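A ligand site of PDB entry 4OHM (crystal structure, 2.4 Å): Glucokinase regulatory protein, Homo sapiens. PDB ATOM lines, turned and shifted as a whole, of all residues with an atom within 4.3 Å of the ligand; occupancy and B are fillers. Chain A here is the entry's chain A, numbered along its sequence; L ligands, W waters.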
ATOM      1  N   VAL A  22       9.322  11.309  13.529  1.00  0.00           N
ATOM      2  CA  VAL A  22       8.007  10.969  14.013  1.00  0.00           C
ATOM      3  C   VAL A  22       7.287  10.336  12.847  1.00  0.00           C
ATOM      4  O   VAL A  22       7.286  10.904  11.796  1.00  0.00           O
ATOM      5  CB  VAL A  22       7.289  12.212  14.559  1.00  0.00           C
ATOM      6  CG1 VAL A  22       5.845  11.928  14.873  1.00  0.00           C
ATOM      7  CG2 VAL A  22       7.952  12.663  15.838  1.00  0.00           C
ATOM      8  N   TYR A  36       2.472   1.185  10.657  1.00  0.00           N
ATOM      9  CA  TYR A  36       2.648   2.139  11.747  1.00  0.00           C
ATOM     10  C   TYR A  36       2.744   1.313  13.015  1.00  0.00           C
ATOM     11  O   TYR A  36       3.700   1.461  13.791  1.00  0.00           O
ATOM     12  CB  TYR A  36       1.503   3.139  11.858  1.00  0.00           C
ATOM     13  CG  TYR A  36       1.651   4.109  13.004  1.00  0.00           C
ATOM     14  CD1 TYR A  36       1.364   3.726  14.301  1.00  0.00           C
ATOM     15  CD2 TYR A  36       2.106   5.385  12.798  1.00  0.00           C
ATOM     16  CE1 TYR A  36       1.517   4.590  15.376  1.00  0.00           C
ATOM     17  CE2 TYR A  36       2.254   6.257  13.873  1.00  0.00           C
ATOM     18  CZ  TYR A  36       1.953   5.856  15.162  1.00  0.00           C
ATOM     19  OH  TYR A  36       2.087   6.711  16.228  1.00  0.00           O
ATOM     20  N   VAL A  40       5.578   0.696  16.562  1.00  0.00           N
ATOM     21  CA  VAL A  40       5.372   1.117  17.956  1.00  0.00           C
ATOM     22  C   VAL A  40       6.123   0.138  18.813  1.00  0.00           C
ATOM     23  O   VAL A  40       5.824  -1.055  18.796  1.00  0.00           O
ATOM     24  CB  VAL A  40       3.889   1.166  18.406  1.00  0.00           C
ATOM     25  CG1 VAL A  40       3.791   1.616  19.876  1.00  0.00           C
ATOM     26  CG2 VAL A  40       3.095   2.127  17.496  1.00  0.00           C
ATOM     27  N   PRO A  41       7.123   0.636  19.574  1.00  0.00           N
ATOM     28  CA  PRO A  41       7.816  -0.298  20.490  1.00  0.00           C
ATOM     29  C   PRO A  41       6.847  -1.078  21.348  1.00  0.00           C
ATOM     30  O   PRO A  41       5.755  -0.583  21.694  1.00  0.00           O
ATOM     31  CB  PRO A  41       8.685   0.612  21.340  1.00  0.00           C
ATOM     32  CG  PRO A  41       8.834   1.876  20.543  1.00  0.00           C
ATOM     33  CD  PRO A  41       7.563   2.026  19.794  1.00  0.00           C
ATOM     34  N   GLU A  44       5.447   0.587  24.437  1.00  0.00           N
ATOM     35  CA  GLU A  44       4.497   1.669  24.319  1.00  0.00           C
ATOM     36  C   GLU A  44       3.181   1.228  23.810  1.00  0.00           C
ATOM     37  O   GLU A  44       2.277   2.022  23.799  1.00  0.00           O
ATOM     38  CB  GLU A  44       5.049   2.744  23.385  1.00  0.00           C
ATOM     39  CG  GLU A  44       6.337   3.359  23.935  1.00  0.00           C
ATOM     40  CD  GLU A  44       6.114   4.305  25.097  1.00  0.00           C
ATOM     41  OE1 GLU A  44       5.050   4.921  25.161  1.00  0.00           O
ATOM     42  OE2 GLU A  44       7.021   4.445  25.956  1.00  0.00           O
ATOM     43  N   LYS A  45       3.053  -0.035  23.423  1.00  0.00           N
ATOM     44  CA  LYS A  45       1.853  -0.497  22.759  1.00  0.00           C
ATOM     45  C   LYS A  45       0.658  -0.495  23.690  1.00  0.00           C
ATOM     46  O   LYS A  45       0.802  -0.558  24.895  1.00  0.00           O
ATOM     47  CB  LYS A  45       2.018  -1.910  22.136  1.00  0.00           C
ATOM     48  CG  LYS A  45       2.625  -1.963  20.723  1.00  0.00           C
ATOM     49  CD  LYS A  45       2.606  -3.397  20.164  1.00  0.00           C
ATOM     50  CE  LYS A  45       3.853  -3.798  19.390  1.00  0.00           C
ATOM     51  NZ  LYS A  45       4.047  -3.024  18.119  1.00  0.00           N
ATOM     52  N   SER A  46      -0.511  -0.389  23.061  1.00  0.00           N
ATOM     53  CA  SER A  46      -1.803  -0.589  23.662  1.00  0.00           C
ATOM     54  C   SER A  46      -2.023  -2.068  23.832  1.00  0.00           C
ATOM     55  O   SER A  46      -2.097  -2.771  22.849  1.00  0.00           O
ATOM     56  CB  SER A  46      -2.903  -0.078  22.697  1.00  0.00           C
ATOM     57  OG  SER A  46      -4.185  -0.477  23.134  1.00  0.00           O
ATOM     58  N   GLY A 193      12.360   0.400  28.167  1.00  0.00           N
ATOM     59  CA  GLY A 193      12.007   0.746  26.828  1.00  0.00           C
ATOM     60  C   GLY A 193      13.216   0.773  25.928  1.00  0.00           C
ATOM     61  O   GLY A 193      13.080   1.107  24.778  1.00  0.00           O
ATOM     62  N   LEU A 194      14.387   0.415  26.446  1.00  0.00           N
ATOM     63  CA  LEU A 194      15.664   0.701  25.773  1.00  0.00           C
ATOM     64  C   LEU A 194      15.566   2.157  25.281  1.00  0.00           C
ATOM     65  O   LEU A 194      15.703   2.444  24.100  1.00  0.00           O
ATOM     66  CB  LEU A 194      15.916  -0.277  24.652  1.00  0.00           C
ATOM     67  CG  LEU A 194      15.960  -1.763  24.984  1.00  0.00           C
ATOM     68  CD1 LEU A 194      16.428  -2.544  23.763  1.00  0.00           C
ATOM     69  CD2 LEU A 194      16.906  -2.016  26.142  1.00  0.00           C
ATOM     70  N   SER A 195      15.282   3.049  26.231  1.00  0.00           N
ATOM     71  CA  SER A 195      14.933   4.414  26.030  1.00  0.00           C
ATOM     72  C   SER A 195      15.833   5.451  26.728  1.00  0.00           C
ATOM     73  O   SER A 195      16.076   6.492  26.151  1.00  0.00           O
ATOM     74  CB  SER A 195      13.508   4.636  26.545  1.00  0.00           C
ATOM     75  OG  SER A 195      13.248   6.023  26.760  1.00  0.00           O
ATOM     76  N   ASN A 221      12.343  -4.485  24.873  1.00  0.00           N
ATOM     77  CA  ASN A 221      12.027  -4.298  23.481  1.00  0.00           C
ATOM     78  C   ASN A 221      13.096  -4.981  22.660  1.00  0.00           C
ATOM     79  O   ASN A 221      14.265  -5.072  23.055  1.00  0.00           O
ATOM     80  CB  ASN A 221      12.001  -2.811  23.106  1.00  0.00           C
ATOM     81  CG  ASN A 221      10.723  -2.099  23.498  1.00  0.00           C
ATOM     82  OD1 ASN A 221       9.618  -2.580  23.233  1.00  0.00           O
ATOM     83  ND2 ASN A 221      10.863  -0.895  24.044  1.00  0.00           N
ATOM     84  N   MET A 225      13.603  -1.957  17.916  1.00  0.00           N
ATOM     85  CA  MET A 225      12.597  -1.031  18.423  1.00  0.00           C
ATOM     86  C   MET A 225      13.189  -0.154  19.497  1.00  0.00           C
ATOM     87  O   MET A 225      12.446   0.512  20.220  1.00  0.00           O
ATOM     88  CB  MET A 225      11.468  -1.814  19.064  1.00  0.00           C
ATOM     89  CG  MET A 225      10.378  -2.270  18.121  1.00  0.00           C
ATOM     90  SD  MET A 225       9.386  -3.555  18.927  1.00  0.00           S
ATOM     91  CE  MET A 225       8.079  -3.690  17.696  1.00  0.00           C
ATOM     92  N   ALA A 226      14.502  -0.204  19.680  1.00  0.00           N
ATOM     93  CA  ALA A 226      15.156   0.608  20.687  1.00  0.00           C
ATOM     94  C   ALA A 226      15.019   2.051  20.285  1.00  0.00           C
ATOM     95  O   ALA A 226      15.030   2.350  19.123  1.00  0.00           O
ATOM     96  CB  ALA A 226      16.602   0.248  20.794  1.00  0.00           C
ATOM     97  N   ARG A 227      14.890   2.931  21.261  1.00  0.00           N
ATOM     98  CA  ARG A 227      14.741   4.381  21.001  1.00  0.00           C
ATOM     99  C   ARG A 227      15.810   4.947  20.058  1.00  0.00           C
ATOM    100  O   ARG A 227      17.015   4.618  20.204  1.00  0.00           O
ATOM    101  CB  ARG A 227      14.724   5.108  22.330  1.00  0.00           C
ATOM    102  CG  ARG A 227      14.250   6.514  22.242  1.00  0.00           C
ATOM    103  CD  ARG A 227      13.832   7.042  23.595  1.00  0.00           C
ATOM    104  NE  ARG A 227      13.584   8.467  23.465  1.00  0.00           N
ATOM    105  CZ  ARG A 227      13.387   9.322  24.465  1.00  0.00           C
ATOM    106  NH1 ARG A 227      13.363   8.942  25.735  1.00  0.00           N
ATOM    107  NH2 ARG A 227      13.202  10.597  24.177  1.00  0.00           N
ATOM    108  N   ASP A 229      15.467   8.564  18.469  1.00  0.00           N
ATOM    109  CA  ASP A 229      15.545  10.033  18.352  1.00  0.00           C
ATOM    110  C   ASP A 229      16.786  10.591  19.094  1.00  0.00           C
ATOM    111  O   ASP A 229      17.208  10.020  20.072  1.00  0.00           O
ATOM    112  CB  ASP A 229      14.281  10.744  18.892  1.00  0.00           C
ATOM    113  CG  ASP A 229      13.985  10.403  20.356  1.00  0.00           C
ATOM    114  OD1 ASP A 229      13.655   9.233  20.636  1.00  0.00           O
ATOM    115  OD2 ASP A 229      14.010  11.280  21.222  1.00  0.00           O
ATOM    116  N   HIS A 516      -5.051   4.308  28.013  1.00  0.00           N
ATOM    117  CA  HIS A 516      -4.086   5.368  27.927  1.00  0.00           C
ATOM    118  C   HIS A 516      -4.313   6.358  29.063  1.00  0.00           C
ATOM    119  O   HIS A 516      -5.472   6.670  29.436  1.00  0.00           O
ATOM    120  CB  HIS A 516      -4.273   6.072  26.590  1.00  0.00           C
ATOM    121  CG  HIS A 516      -3.963   5.207  25.407  1.00  0.00           C
ATOM    122  ND1 HIS A 516      -2.715   4.672  25.191  1.00  0.00           N
ATOM    123  CD2 HIS A 516      -4.733   4.810  24.370  1.00  0.00           C
ATOM    124  CE1 HIS A 516      -2.734   3.971  24.068  1.00  0.00           C
ATOM    125  NE2 HIS A 516      -3.937   4.053  23.544  1.00  0.00           N
ATOM    126  N   LYS A 526      10.541  11.488  26.578  1.00  0.00           N
ATOM    127  CA  LYS A 526       9.710  10.329  26.271  1.00  0.00           C
ATOM    128  C   LYS A 526       8.209  10.586  26.460  1.00  0.00           C
ATOM    129  O   LYS A 526       7.379  10.213  25.650  1.00  0.00           O
ATOM    130  CB  LYS A 526      10.147   9.142  27.112  1.00  0.00           C
ATOM    131  CG  LYS A 526       9.285   7.901  26.940  1.00  0.00           C
ATOM    132  CD  LYS A 526       9.901   6.732  27.709  1.00  0.00           C
ATOM    133  CE  LYS A 526       9.899   6.959  29.222  1.00  0.00           C
ATOM    134  NZ  LYS A 526      10.362   5.718  29.861  1.00  0.00           N
ATOM    135  N   TRP A 529       7.016  12.713  23.680  1.00  0.00           N
ATOM    136  CA  TRP A 529       6.665  11.876  22.503  1.00  0.00           C
ATOM    137  C   TRP A 529       5.363  11.087  22.670  1.00  0.00           C
ATOM    138  O   TRP A 529       4.579  10.983  21.725  1.00  0.00           O
ATOM    139  CB  TRP A 529       7.794  10.974  22.114  1.00  0.00           C
ATOM    140  CG  TRP A 529       9.022  11.748  21.731  1.00  0.00           C
ATOM    141  CD1 TRP A 529      10.223  11.651  22.304  1.00  0.00           C
ATOM    142  CD2 TRP A 529       9.127  12.743  20.693  1.00  0.00           C
ATOM    143  NE1 TRP A 529      11.121  12.494  21.668  1.00  0.00           N
ATOM    144  CE2 TRP A 529      10.465  13.181  20.678  1.00  0.00           C
ATOM    145  CE3 TRP A 529       8.231  13.258  19.747  1.00  0.00           C
ATOM    146  CZ2 TRP A 529      10.948  14.149  19.798  1.00  0.00           C
ATOM    147  CZ3 TRP A 529       8.700  14.244  18.819  1.00  0.00           C
ATOM    148  CH2 TRP A 529      10.048  14.683  18.875  1.00  0.00           C
ATOM    149  N   ARG A 530       5.134  10.560  23.867  1.00  0.00           N
ATOM    150  CA  ARG A 530       3.912   9.817  24.153  1.00  0.00           C
ATOM    151  C   ARG A 530       2.661  10.706  24.069  1.00  0.00           C
ATOM    152  O   ARG A 530       1.602  10.274  23.575  1.00  0.00           O
ATOM    153  CB  ARG A 530       4.007   9.133  25.517  1.00  0.00           C
ATOM    154  CG  ARG A 530       2.850   8.184  25.841  1.00  0.00           C
ATOM    155  CD  ARG A 530       3.055   7.490  27.186  1.00  0.00           C
ATOM    156  NE  ARG A 530       4.305   6.716  27.229  1.00  0.00           N
ATOM    157  CZ  ARG A 530       5.042   6.461  28.316  1.00  0.00           C
ATOM    158  NH1 ARG A 530       4.679   6.936  29.497  1.00  0.00           N
ATOM    159  NH2 ARG A 530       6.167   5.730  28.231  1.00  0.00           N
ATOM    160  N   ALA A 533       2.010  11.097  20.263  1.00  0.00           N
ATOM    161  CA  ALA A 533       1.385   9.887  19.753  1.00  0.00           C
ATOM    162  C   ALA A 533      -0.065   9.742  20.155  1.00  0.00           C
ATOM    163  O   ALA A 533      -0.898   9.263  19.372  1.00  0.00           O
ATOM    164  CB  ALA A 533       2.151   8.667  20.231  1.00  0.00           C
ATOM    165  N   MET A 534      -0.366  10.088  21.398  1.00  0.00           N
ATOM    166  CA  MET A 534      -1.749   9.974  21.854  1.00  0.00           C
ATOM    167  C   MET A 534      -2.591  10.990  21.110  1.00  0.00           C
ATOM    168  O   MET A 534      -3.697  10.654  20.685  1.00  0.00           O
ATOM    169  CB  MET A 534      -1.846  10.142  23.332  1.00  0.00           C
ATOM    170  CG  MET A 534      -1.450   8.895  24.068  1.00  0.00           C
ATOM    171  SD  MET A 534      -1.837   9.146  25.791  1.00  0.00           S
ATOM    172  CE  MET A 534      -0.687  10.404  26.299  1.00  0.00           C
ATOM    173  N   GLN A 536      -2.005  12.014  17.875  1.00  0.00           N
ATOM    174  CA  GLN A 536      -2.257  11.443  16.521  1.00  0.00           C
ATOM    175  C   GLN A 536      -3.371  10.390  16.512  1.00  0.00           C
ATOM    176  O   GLN A 536      -4.252  10.399  15.657  1.00  0.00           O
ATOM    177  CB  GLN A 536      -0.983  10.807  15.958  1.00  0.00           C
ATOM    178  CG  GLN A 536       0.090  11.822  15.665  1.00  0.00           C
ATOM    179  CD  GLN A 536       1.448  11.227  15.341  1.00  0.00           C
ATOM    180  OE1 GLN A 536       2.330  11.184  16.207  1.00  0.00           O
ATOM    181  NE2 GLN A 536       1.645  10.804  14.089  1.00  0.00           N
ATOM    182  N   ARG A 537      -3.329   9.475  17.467  1.00  0.00           N
ATOM    183  CA  ARG A 537      -4.234   8.345  17.557  1.00  0.00           C
ATOM    184  C   ARG A 537      -5.680   8.796  17.819  1.00  0.00           C
ATOM    185  O   ARG A 537      -6.602   8.367  17.144  1.00  0.00           O
ATOM    186  CB  ARG A 537      -3.747   7.426  18.689  1.00  0.00           C
ATOM    187  CG  ARG A 537      -4.647   6.246  19.087  1.00  0.00           C
ATOM    188  CD  ARG A 537      -4.513   5.034  18.215  1.00  0.00           C
ATOM    189  NE  ARG A 537      -3.207   4.385  18.354  1.00  0.00           N
ATOM    190  CZ  ARG A 537      -2.813   3.346  17.623  1.00  0.00           C
ATOM    191  NH1 ARG A 537      -3.615   2.824  16.711  1.00  0.00           N
ATOM    192  NH2 ARG A 537      -1.612   2.820  17.803  1.00  0.00           N
HETATM  193  C1  LIG L   1      10.410   5.311  23.527  1.00  0.00           C
HETATM  194  C2  LIG L   1      10.870   4.010  23.601  1.00  0.00           C
HETATM  195  C3  LIG L   1      11.402   3.450  22.462  1.00  0.00           C
HETATM  196  N1  LIG L   1      11.883   2.220  22.506  1.00  0.00           N
HETATM  197  N2  LIG L   1      11.462   4.149  21.273  1.00  0.00           N
HETATM  198  C4  LIG L   1      11.010   5.376  21.180  1.00  0.00           C
HETATM  199  C5  LIG L   1      10.470   5.999  22.317  1.00  0.00           C
HETATM  200  S1  LIG L   1       9.797   7.601  22.145  1.00  0.00           S
HETATM  201  O1  LIG L   1      10.398   8.154  20.919  1.00  0.00           O
HETATM  202  O2  LIG L   1      10.023   8.381  23.364  1.00  0.00           O
HETATM  203  N3  LIG L   1       8.241   7.475  21.836  1.00  0.00           N
HETATM  204  C6  LIG L   1       8.054   6.492  20.766  1.00  0.00           C
HETATM  205  C7  LIG L   1       6.564   6.409  20.320  1.00  0.00           C
HETATM  206  C8  LIG L   1       6.274   7.718  19.663  1.00  0.00           C
HETATM  207  C9  LIG L   1       5.979   8.758  19.134  1.00  0.00           C
HETATM  208  C10 LIG L   1       5.724  10.072  18.528  1.00  0.00           C
HETATM  209  C11 LIG L   1       7.504   6.980  22.977  1.00  0.00           C
HETATM  210  C12 LIG L   1       5.990   7.080  22.658  1.00  0.00           C
HETATM  211  N4  LIG L   1       5.648   6.341  21.438  1.00  0.00           N
HETATM  212  C13 LIG L   1       4.325   5.945  21.265  1.00  0.00           C
HETATM  213  C14 LIG L   1       3.842   5.698  20.020  1.00  0.00           C
HETATM  214  C15 LIG L   1       2.512   5.333  19.842  1.00  0.00           C
HETATM  215  C16 LIG L   1       3.439   5.794  22.335  1.00  0.00           C
HETATM  216  C17 LIG L   1       2.112   5.407  22.162  1.00  0.00           C
HETATM  217  C18 LIG L   1       1.642   5.169  20.890  1.00  0.00           C
HETATM  218  C19 LIG L   1       0.199   4.817  20.625  1.00  0.00           C
HETATM  219  C20 LIG L   1      -0.129   3.392  21.036  1.00  0.00           C
HETATM  220  F1  LIG L   1       0.650   2.608  20.327  1.00  0.00           F
HETATM  221  F2  LIG L   1      -0.044   3.347  22.390  1.00  0.00           F
HETATM  222  F3  LIG L   1      -1.362   3.031  20.684  1.00  0.00           F
HETATM  223  O3  LIG L   1      -0.080   4.979  19.239  1.00  0.00           O
HETATM  224  C21 LIG L   1      -0.684   5.855  21.286  1.00  0.00           C
HETATM  225  O4  LIG L   1      -2.000   5.585  20.753  1.00  0.00           O
HETATM  226  O   HOH W   1       9.118   2.804  26.350  1.00  0.00           O
HETATM  227  O   HOH W   2      -0.071   7.209  17.841  1.00  0.00           O
HETATM  228  O   HOH W   3      11.187   3.451  18.604  1.00  0.00           O
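The backbone carbonyl oxygen (O) of Gly 193 is in hydrogen-bond range of a nitrogen (N1) of the ligand (2.8 Å). The guanidinium group (NE) of Arg 537 sits at hydrogen-bond distance from an oxygen (O4) of the ligand (2.9 Å). The backbone carbonyl oxygen (O) of Met 225 lies within hydrogen-bond range of a nitrogen (N1) of the ligand (2.9 Å).
The side-chain amide nitrogen (ND2) of Asn 221 lies within hydrogen-bond range of the backbone carbonyl oxygen (O) of Gly 193 (3.1 Å). The side-chain carboxylate (OE2) of Glu 44 lies within salt-bridge range of the guanidinium group (NH2) of Arg 530 (2.7 Å). The side-chain carboxylate of Asp 229 is in salt-bridge range of the guanidinium group of Arg 227 (2.9 Å). NH1 of Arg 227 lies within hydrogen-bond range of OG of Ser 195 (3.1 Å). N of Arg 227 sits at hydrogen-bond distance from O of Leu 194, at 3.0 Å. The backbone carbonyl oxygen of Val 40 is in hydrogen-bond range of the side-chain amino group of Lys 45 (2.7 Å). The side-chain carboxylate of Asp 229 lies within hydrogen-bond range of the indole nitrogen of Trp 529, at 3.2 Å.
O of Glu 44 lies close to F2 of the ligand, 3.0 Å away. A nitrogen (N1) of the ligand sits close to the backbone NH (N) of Arg 227 (3.3 Å). O1 of the ligand lies close to OD1 of Asp 229. OH of Tyr 36 touches C15 of the ligand (3.9 Å). CG1 of Val 40 touches F1 of the ligand, at 3.3 Å. Pro 41 touches the ligand (CG to N2, 3.6 Å). Ser 46 touches the ligand. ND2 of Asn 221 touches N1 of the ligand, at 3.6 Å. C of Ala 226 touches N1 of the ligand, at 3.8 Å. His 516 touches the ligand. Lys 526 touches the ligand (CA to O2, 3.5 Å). CD1 of Trp 529 touches O2 of the ligand (3.4 Å). CA of Arg 530 touches C12 of the ligand, 3.7 Å away. CB of Ala 533 touches C15 of the ligand (3.4 Å). Hydrophobic or aromatic side chains that line the ligand: Val 40, Pro 41, His 516, Trp 529 and Ala 533. Within 4 Å of the ligand: Tyr 36, Val 40, Pro 41, Glu 44, Ser 46, Gly 193, Asn 221, Met 225, Ala 226, Arg 227, Asp 229, His 516, Lys 526, Trp 529, Arg 530, Ala 533 and Arg 537. The nearest printed residue that does not touch the ligand is Ser 195 (4.002 Å).
Water W2 lies within hydrogen-bond range of an oxygen (O3) of the ligand (2.6 Å), the backbone carbonyl oxygen (O) of Ala 533 (2.7 Å) and the side-chain hydroxyl (OH) of Tyr 36 (2.7 Å).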
